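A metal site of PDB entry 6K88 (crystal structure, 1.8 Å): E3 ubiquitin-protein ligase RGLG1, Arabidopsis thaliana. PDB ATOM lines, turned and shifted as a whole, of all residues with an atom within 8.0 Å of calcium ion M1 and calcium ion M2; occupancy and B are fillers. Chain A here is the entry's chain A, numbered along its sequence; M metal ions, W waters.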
ATOM      1  N   ILE A 199     -13.995  19.968  -1.264  1.00  0.00           N
ATOM      2  CA  ILE A 199     -14.296  19.028  -2.325  1.00  0.00           C
ATOM      3  C   ILE A 199     -13.068  18.821  -3.200  1.00  0.00           C
ATOM      4  O   ILE A 199     -12.426  19.787  -3.635  1.00  0.00           O
ATOM      5  CB  ILE A 199     -15.484  19.497  -3.202  1.00  0.00           C
ATOM      6  CG1 ILE A 199     -16.692  19.800  -2.336  1.00  0.00           C
ATOM      7  CG2 ILE A 199     -15.810  18.446  -4.277  1.00  0.00           C
ATOM      8  CD1 ILE A 199     -17.777  20.606  -3.061  1.00  0.00           C
ATOM      9  N   MET A 212     -13.846  20.938 -15.021  1.00  0.00           N
ATOM     10  CA  MET A 212     -13.328  20.717 -13.662  1.00  0.00           C
ATOM     11  C   MET A 212     -12.419  21.865 -13.267  1.00  0.00           C
ATOM     12  O   MET A 212     -12.432  22.304 -12.110  1.00  0.00           O
ATOM     13  CB  MET A 212     -12.576  19.379 -13.562  1.00  0.00           C
ATOM     14  CG  MET A 212     -13.418  18.136 -13.921  1.00  0.00           C
ATOM     15  SD  MET A 212     -14.973  17.978 -13.012  1.00  0.00           S
ATOM     16  CE  MET A 212     -16.159  18.665 -14.147  1.00  0.00           C
ATOM     17  N   GLN A 213     -11.613  22.355 -14.219  1.00  0.00           N
ATOM     18  CA  GLN A 213     -10.704  23.463 -13.941  1.00  0.00           C
ATOM     19  C   GLN A 213     -11.504  24.729 -13.624  1.00  0.00           C
ATOM     20  O   GLN A 213     -11.099  25.552 -12.801  1.00  0.00           O
ATOM     21  CB  GLN A 213      -9.759  23.691 -15.120  1.00  0.00           C
ATOM     22  CG  GLN A 213      -8.587  22.713 -15.146  1.00  0.00           C
ATOM     23  CD  GLN A 213      -7.950  22.572 -16.524  1.00  0.00           C
ATOM     24  OE1 GLN A 213      -8.450  23.105 -17.510  1.00  0.00           O
ATOM     25  NE2 GLN A 213      -6.843  21.833 -16.591  1.00  0.00           N
ATOM     26  N   GLU A 214     -12.657  24.854 -14.268  1.00  0.00           N
ATOM     27  CA  GLU A 214     -13.562  25.949 -13.967  1.00  0.00           C
ATOM     28  C   GLU A 214     -14.187  25.826 -12.576  1.00  0.00           C
ATOM     29  O   GLU A 214     -14.285  26.828 -11.874  1.00  0.00           O
ATOM     30  CB  GLU A 214     -14.673  26.021 -15.025  1.00  0.00           C
ATOM     31  CG  GLU A 214     -15.736  27.047 -14.718  1.00  0.00           C
ATOM     32  CD  GLU A 214     -16.002  27.985 -15.878  1.00  0.00           C
ATOM     33  OE1 GLU A 214     -15.029  28.404 -16.553  1.00  0.00           O
ATOM     34  OE2 GLU A 214     -17.189  28.309 -16.119  1.00  0.00           O
ATOM     35  N   PHE A 215     -14.611  24.621 -12.177  1.00  0.00           N
ATOM     36  CA  PHE A 215     -15.120  24.441 -10.810  1.00  0.00           C
ATOM     37  C   PHE A 215     -14.009  24.727  -9.794  1.00  0.00           C
ATOM     38  O   PHE A 215     -14.257  25.289  -8.718  1.00  0.00           O
ATOM     39  CB  PHE A 215     -15.686  23.023 -10.579  1.00  0.00           C
ATOM     40  CG  PHE A 215     -16.921  22.692 -11.387  1.00  0.00           C
ATOM     41  CD1 PHE A 215     -17.693  23.687 -11.977  1.00  0.00           C
ATOM     42  CD2 PHE A 215     -17.316  21.356 -11.552  1.00  0.00           C
ATOM     43  CE1 PHE A 215     -18.834  23.363 -12.721  1.00  0.00           C
ATOM     44  CE2 PHE A 215     -18.458  21.033 -12.282  1.00  0.00           C
ATOM     45  CZ  PHE A 215     -19.200  22.025 -12.872  1.00  0.00           C
ATOM     46  N   ASP A 216     -12.786  24.333 -10.157  1.00  0.00           N
ATOM     47  CA  ASP A 216     -11.605  24.529  -9.325  1.00  0.00           C
ATOM     48  C   ASP A 216     -11.321  26.028  -9.115  1.00  0.00           C
ATOM     49  O   ASP A 216     -11.119  26.475  -7.987  1.00  0.00           O
ATOM     50  CB  ASP A 216     -10.389  23.842  -9.977  1.00  0.00           C
ATOM     51  CG  ASP A 216      -9.141  23.822  -9.085  1.00  0.00           C
ATOM     52  OD1 ASP A 216      -9.098  24.473  -8.023  1.00  0.00           O
ATOM     53  OD2 ASP A 216      -8.168  23.139  -9.469  1.00  0.00           O
ATOM     54  N   ASP A 217     -11.334  26.794 -10.211  1.00  0.00           N
ATOM     55  CA  ASP A 217     -10.739  28.135 -10.201  1.00  0.00           C
ATOM     56  C   ASP A 217     -11.724  29.292 -10.316  1.00  0.00           C
ATOM     57  O   ASP A 217     -11.395  30.428  -9.993  1.00  0.00           O
ATOM     58  CB  ASP A 217      -9.714  28.273 -11.330  1.00  0.00           C
ATOM     59  CG  ASP A 217      -8.558  27.282 -11.207  1.00  0.00           C
ATOM     60  OD1 ASP A 217      -8.139  26.946 -10.073  1.00  0.00           O
ATOM     61  OD2 ASP A 217      -8.039  26.869 -12.265  1.00  0.00           O
ATOM     62  N   ASN A 218     -12.946  29.022 -10.780  1.00  0.00           N
ATOM     63  CA  ASN A 218     -13.795  30.100 -11.264  1.00  0.00           C
ATOM     64  C   ASN A 218     -15.279  29.975 -10.925  1.00  0.00           C
ATOM     65  O   ASN A 218     -16.118  29.837 -11.810  1.00  0.00           O
ATOM     66  CB  ASN A 218     -13.631  30.226 -12.777  1.00  0.00           C
ATOM     67  CG  ASN A 218     -14.198  31.522 -13.320  1.00  0.00           C
ATOM     68  OD1 ASN A 218     -14.376  32.496 -12.589  1.00  0.00           O
ATOM     69  ND2 ASN A 218     -14.498  31.533 -14.613  1.00  0.00           N
ATOM     70  N   ARG A 222     -19.023  32.080  -4.334  1.00  0.00           N
ATOM     71  CA  ARG A 222     -18.479  31.121  -3.370  1.00  0.00           C
ATOM     72  C   ARG A 222     -17.926  31.779  -2.094  1.00  0.00           C
ATOM     73  O   ARG A 222     -17.237  32.783  -2.185  1.00  0.00           O
ATOM     74  CB  ARG A 222     -17.380  30.340  -4.079  1.00  0.00           C
ATOM     75  CG  ARG A 222     -17.047  29.056  -3.453  1.00  0.00           C
ATOM     76  CD  ARG A 222     -16.476  28.092  -4.475  1.00  0.00           C
ATOM     77  NE  ARG A 222     -15.258  28.549  -5.146  1.00  0.00           N
ATOM     78  CZ  ARG A 222     -14.576  27.771  -5.977  1.00  0.00           C
ATOM     79  NH1 ARG A 222     -15.017  26.534  -6.186  1.00  0.00           N
ATOM     80  NH2 ARG A 222     -13.482  28.203  -6.589  1.00  0.00           N
ATOM     81  N   PHE A 224     -15.649  30.438   0.102  1.00  0.00           N
ATOM     82  CA  PHE A 224     -14.214  30.242   0.029  1.00  0.00           C
ATOM     83  C   PHE A 224     -13.936  29.250  -1.098  1.00  0.00           C
ATOM     84  O   PHE A 224     -14.872  28.605  -1.568  1.00  0.00           O
ATOM     85  CB  PHE A 224     -13.643  29.743   1.368  1.00  0.00           C
ATOM     86  CG  PHE A 224     -13.892  28.281   1.645  1.00  0.00           C
ATOM     87  CD1 PHE A 224     -15.138  27.836   2.039  1.00  0.00           C
ATOM     88  CD2 PHE A 224     -12.864  27.354   1.529  1.00  0.00           C
ATOM     89  CE1 PHE A 224     -15.369  26.481   2.307  1.00  0.00           C
ATOM     90  CE2 PHE A 224     -13.081  26.002   1.798  1.00  0.00           C
ATOM     91  CZ  PHE A 224     -14.330  25.567   2.190  1.00  0.00           C
ATOM     92  N   ASP A 225     -12.700  29.131  -1.546  1.00  0.00           N
ATOM     93  CA  ASP A 225     -12.353  28.162  -2.590  1.00  0.00           C
ATOM     94  C   ASP A 225     -12.453  26.737  -2.039  1.00  0.00           C
ATOM     95  O   ASP A 225     -11.505  26.216  -1.470  1.00  0.00           O
ATOM     96  CB  ASP A 225     -10.940  28.419  -3.131  1.00  0.00           C
ATOM     97  CG  ASP A 225     -10.584  27.552  -4.346  1.00  0.00           C
ATOM     98  OD1 ASP A 225     -11.373  26.661  -4.725  1.00  0.00           O
ATOM     99  OD2 ASP A 225      -9.485  27.753  -4.905  1.00  0.00           O
ATOM    100  N   ASN A 226     -13.616  26.111  -2.234  1.00  0.00           N
ATOM    101  CA  ASN A 226     -13.874  24.774  -1.654  1.00  0.00           C
ATOM    102  C   ASN A 226     -13.802  23.619  -2.656  1.00  0.00           C
ATOM    103  O   ASN A 226     -14.259  22.511  -2.357  1.00  0.00           O
ATOM    104  CB  ASN A 226     -15.257  24.760  -1.004  1.00  0.00           C
ATOM    105  CG  ASN A 226     -16.377  24.935  -2.028  1.00  0.00           C
ATOM    106  OD1 ASN A 226     -16.166  25.436  -3.131  1.00  0.00           O
ATOM    107  ND2 ASN A 226     -17.571  24.512  -1.651  1.00  0.00           N
ATOM    108  N   PHE A 227     -13.243  23.877  -3.838  1.00  0.00           N
ATOM    109  CA  PHE A 227     -13.181  22.850  -4.871  1.00  0.00           C
ATOM    110  C   PHE A 227     -11.775  22.772  -5.457  1.00  0.00           C
ATOM    111  O   PHE A 227     -11.258  23.763  -5.980  1.00  0.00           O
ATOM    112  CB  PHE A 227     -14.196  23.158  -5.969  1.00  0.00           C
ATOM    113  CG  PHE A 227     -14.467  22.008  -6.908  1.00  0.00           C
ATOM    114  CD1 PHE A 227     -13.533  21.631  -7.868  1.00  0.00           C
ATOM    115  CD2 PHE A 227     -15.679  21.337  -6.865  1.00  0.00           C
ATOM    116  CE1 PHE A 227     -13.795  20.600  -8.753  1.00  0.00           C
ATOM    117  CE2 PHE A 227     -15.952  20.293  -7.749  1.00  0.00           C
ATOM    118  CZ  PHE A 227     -15.003  19.912  -8.681  1.00  0.00           C
ATOM    119  N   GLN A 228     -11.165  21.596  -5.356  1.00  0.00           N
ATOM    120  CA  GLN A 228      -9.852  21.331  -5.934  1.00  0.00           C
ATOM    121  C   GLN A 228      -9.925  20.257  -7.021  1.00  0.00           C
ATOM    122  O   GLN A 228     -10.599  19.231  -6.850  1.00  0.00           O
ATOM    123  CB  GLN A 228      -8.857  20.924  -4.843  1.00  0.00           C
ATOM    124  CG  GLN A 228      -7.577  20.225  -5.324  1.00  0.00           C
ATOM    125  CD  GLN A 228      -6.596  21.184  -5.978  1.00  0.00           C
ATOM    126  OE1 GLN A 228      -6.996  22.139  -6.635  1.00  0.00           O
ATOM    127  NE2 GLN A 228      -5.310  20.931  -5.784  1.00  0.00           N
ATOM    128  N   PHE A 229      -9.258  20.494  -8.144  1.00  0.00           N
ATOM    129  CA  PHE A 229      -9.127  19.484  -9.192  1.00  0.00           C
ATOM    130  C   PHE A 229      -7.731  18.851  -9.188  1.00  0.00           C
ATOM    131  O   PHE A 229      -6.732  19.563  -9.234  1.00  0.00           O
ATOM    132  CB  PHE A 229      -9.439  20.083 -10.573  1.00  0.00           C
ATOM    133  CG  PHE A 229      -9.042  19.201 -11.723  1.00  0.00           C
ATOM    134  CD1 PHE A 229      -9.660  17.975 -11.905  1.00  0.00           C
ATOM    135  CD2 PHE A 229      -8.057  19.584 -12.616  1.00  0.00           C
ATOM    136  CE1 PHE A 229      -9.286  17.135 -12.959  1.00  0.00           C
ATOM    137  CE2 PHE A 229      -7.686  18.755 -13.670  1.00  0.00           C
ATOM    138  CZ  PHE A 229      -8.307  17.539 -13.839  1.00  0.00           C
ATOM    139  N   VAL A 230      -7.680  17.518  -9.105  1.00  0.00           N
ATOM    140  CA  VAL A 230      -6.437  16.782  -9.292  1.00  0.00           C
ATOM    141  C   VAL A 230      -6.567  15.822 -10.458  1.00  0.00           C
ATOM    142  O   VAL A 230      -7.479  14.981 -10.487  1.00  0.00           O
ATOM    143  CB  VAL A 230      -6.055  15.972  -8.043  1.00  0.00           C
ATOM    144  CG1 VAL A 230      -4.732  15.231  -8.265  1.00  0.00           C
ATOM    145  CG2 VAL A 230      -5.950  16.887  -6.838  1.00  0.00           C
ATOM    146  N   SER A 252      -1.372  17.182  -3.629  1.00  0.00           N
ATOM    147  CA  SER A 252      -2.200  17.961  -4.557  1.00  0.00           C
ATOM    148  C   SER A 252      -3.639  17.960  -4.100  1.00  0.00           C
ATOM    149  O   SER A 252      -4.293  18.989  -4.097  1.00  0.00           O
ATOM    150  CB  SER A 252      -2.111  17.406  -5.982  1.00  0.00           C
ATOM    151  OG  SER A 252      -0.829  17.631  -6.528  1.00  0.00           O
ATOM    152  N   MET A 255      -3.967  20.305  -1.235  1.00  0.00           N
ATOM    153  CA  MET A 255      -3.321  21.599  -1.448  1.00  0.00           C
ATOM    154  C   MET A 255      -4.190  22.794  -1.041  1.00  0.00           C
ATOM    155  O   MET A 255      -3.686  23.764  -0.491  1.00  0.00           O
ATOM    156  CB  MET A 255      -2.903  21.729  -2.911  1.00  0.00           C
ATOM    157  CG  MET A 255      -2.137  23.001  -3.250  1.00  0.00           C
ATOM    158  SD  MET A 255      -0.508  23.055  -2.456  1.00  0.00           S
ATOM    159  CE  MET A 255       0.226  21.559  -3.124  1.00  0.00           C
ATOM    160  N   GLU A 256      -5.490  22.709  -1.286  1.00  0.00           N
ATOM    161  CA  GLU A 256      -6.399  23.821  -1.014  1.00  0.00           C
ATOM    162  C   GLU A 256      -7.205  23.688   0.271  1.00  0.00           C
ATOM    163  O   GLU A 256      -8.184  24.417   0.474  1.00  0.00           O
ATOM    164  CB  GLU A 256      -7.377  23.999  -2.179  1.00  0.00           C
ATOM    165  CG  GLU A 256      -6.705  24.200  -3.512  1.00  0.00           C
ATOM    166  CD  GLU A 256      -7.682  24.590  -4.602  1.00  0.00           C
ATOM    167  OE1 GLU A 256      -8.905  24.616  -4.324  1.00  0.00           O
ATOM    168  OE2 GLU A 256      -7.240  24.887  -5.724  1.00  0.00           O
HETATM  169 CA    CA M   1      -6.580  24.024  -7.818  1.00  0.00          CA
HETATM  170 CA    CA M   2      -9.764  25.673  -6.218  1.00  0.00          CA
HETATM  171  O   HOH W   1      -5.345  22.525  -9.009  1.00  0.00           O
HETATM  172  O   HOH W   2      -8.314  27.283  -7.369  1.00  0.00           O
HETATM  173  O   HOH W   3      -4.342  24.395  -6.947  1.00  0.00           O
HETATM  174  O   HOH W   4      -5.945  25.564  -9.582  1.00  0.00           O
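The side-chain amide nitrogen (NE2) of Gln 228 lies within hydrogen-bond range of the backbone carbonyl oxygen (O) of Ser 252, at 2.8 Å. The backbone NH (N) of Phe 229 lies close to the side-chain carboxylate (OD2) of Asp 216 (3.2 Å). OD1 of Asp 225 sits close to NH2 of Arg 222 (3.2 Å). The backbone NH (N) of Gln 228 lies within hydrogen-bond range of the backbone carbonyl oxygen (O) of Ile 199 (2.8 Å). The guanidinium group (NH2) of Arg 222 lies close to the backbone carbonyl oxygen (O) of Asp 216 (3.2 Å).
Calcium ion M1 is bound by OE1 of Gln 228 (2.3 Å), water W1 (2.3 Å), OE2 of Glu 256 (2.4 Å), water W4 (2.4 Å), water W3 (2.4 Å), OD2 of Asp 216 (2.5 Å) and OD1 of Asp 216 (2.6 Å).
Calcium ion M2 is bound by OD1 of Asp 216 (2.3 Å), OE1 of Glu 256 (2.3 Å), O of Asp 216 (2.4 Å), OD1 of Asp 225 (2.4 Å), O of Phe 227 (2.4 Å), water W2 (2.5 Å), OD2 of Asp 225 (2.5 Å) and OE2 of Glu 256 (2.7 Å). Calcium ion M2 has eight donor atoms within binding distance.
Along chain A the residues within 4 Å of calcium ion M1 span positions 216 to 256.
Four residues have an atom within 4 Å of calcium ion M2: Asp 216, Asp 225, Phe 227 and Glu 256.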
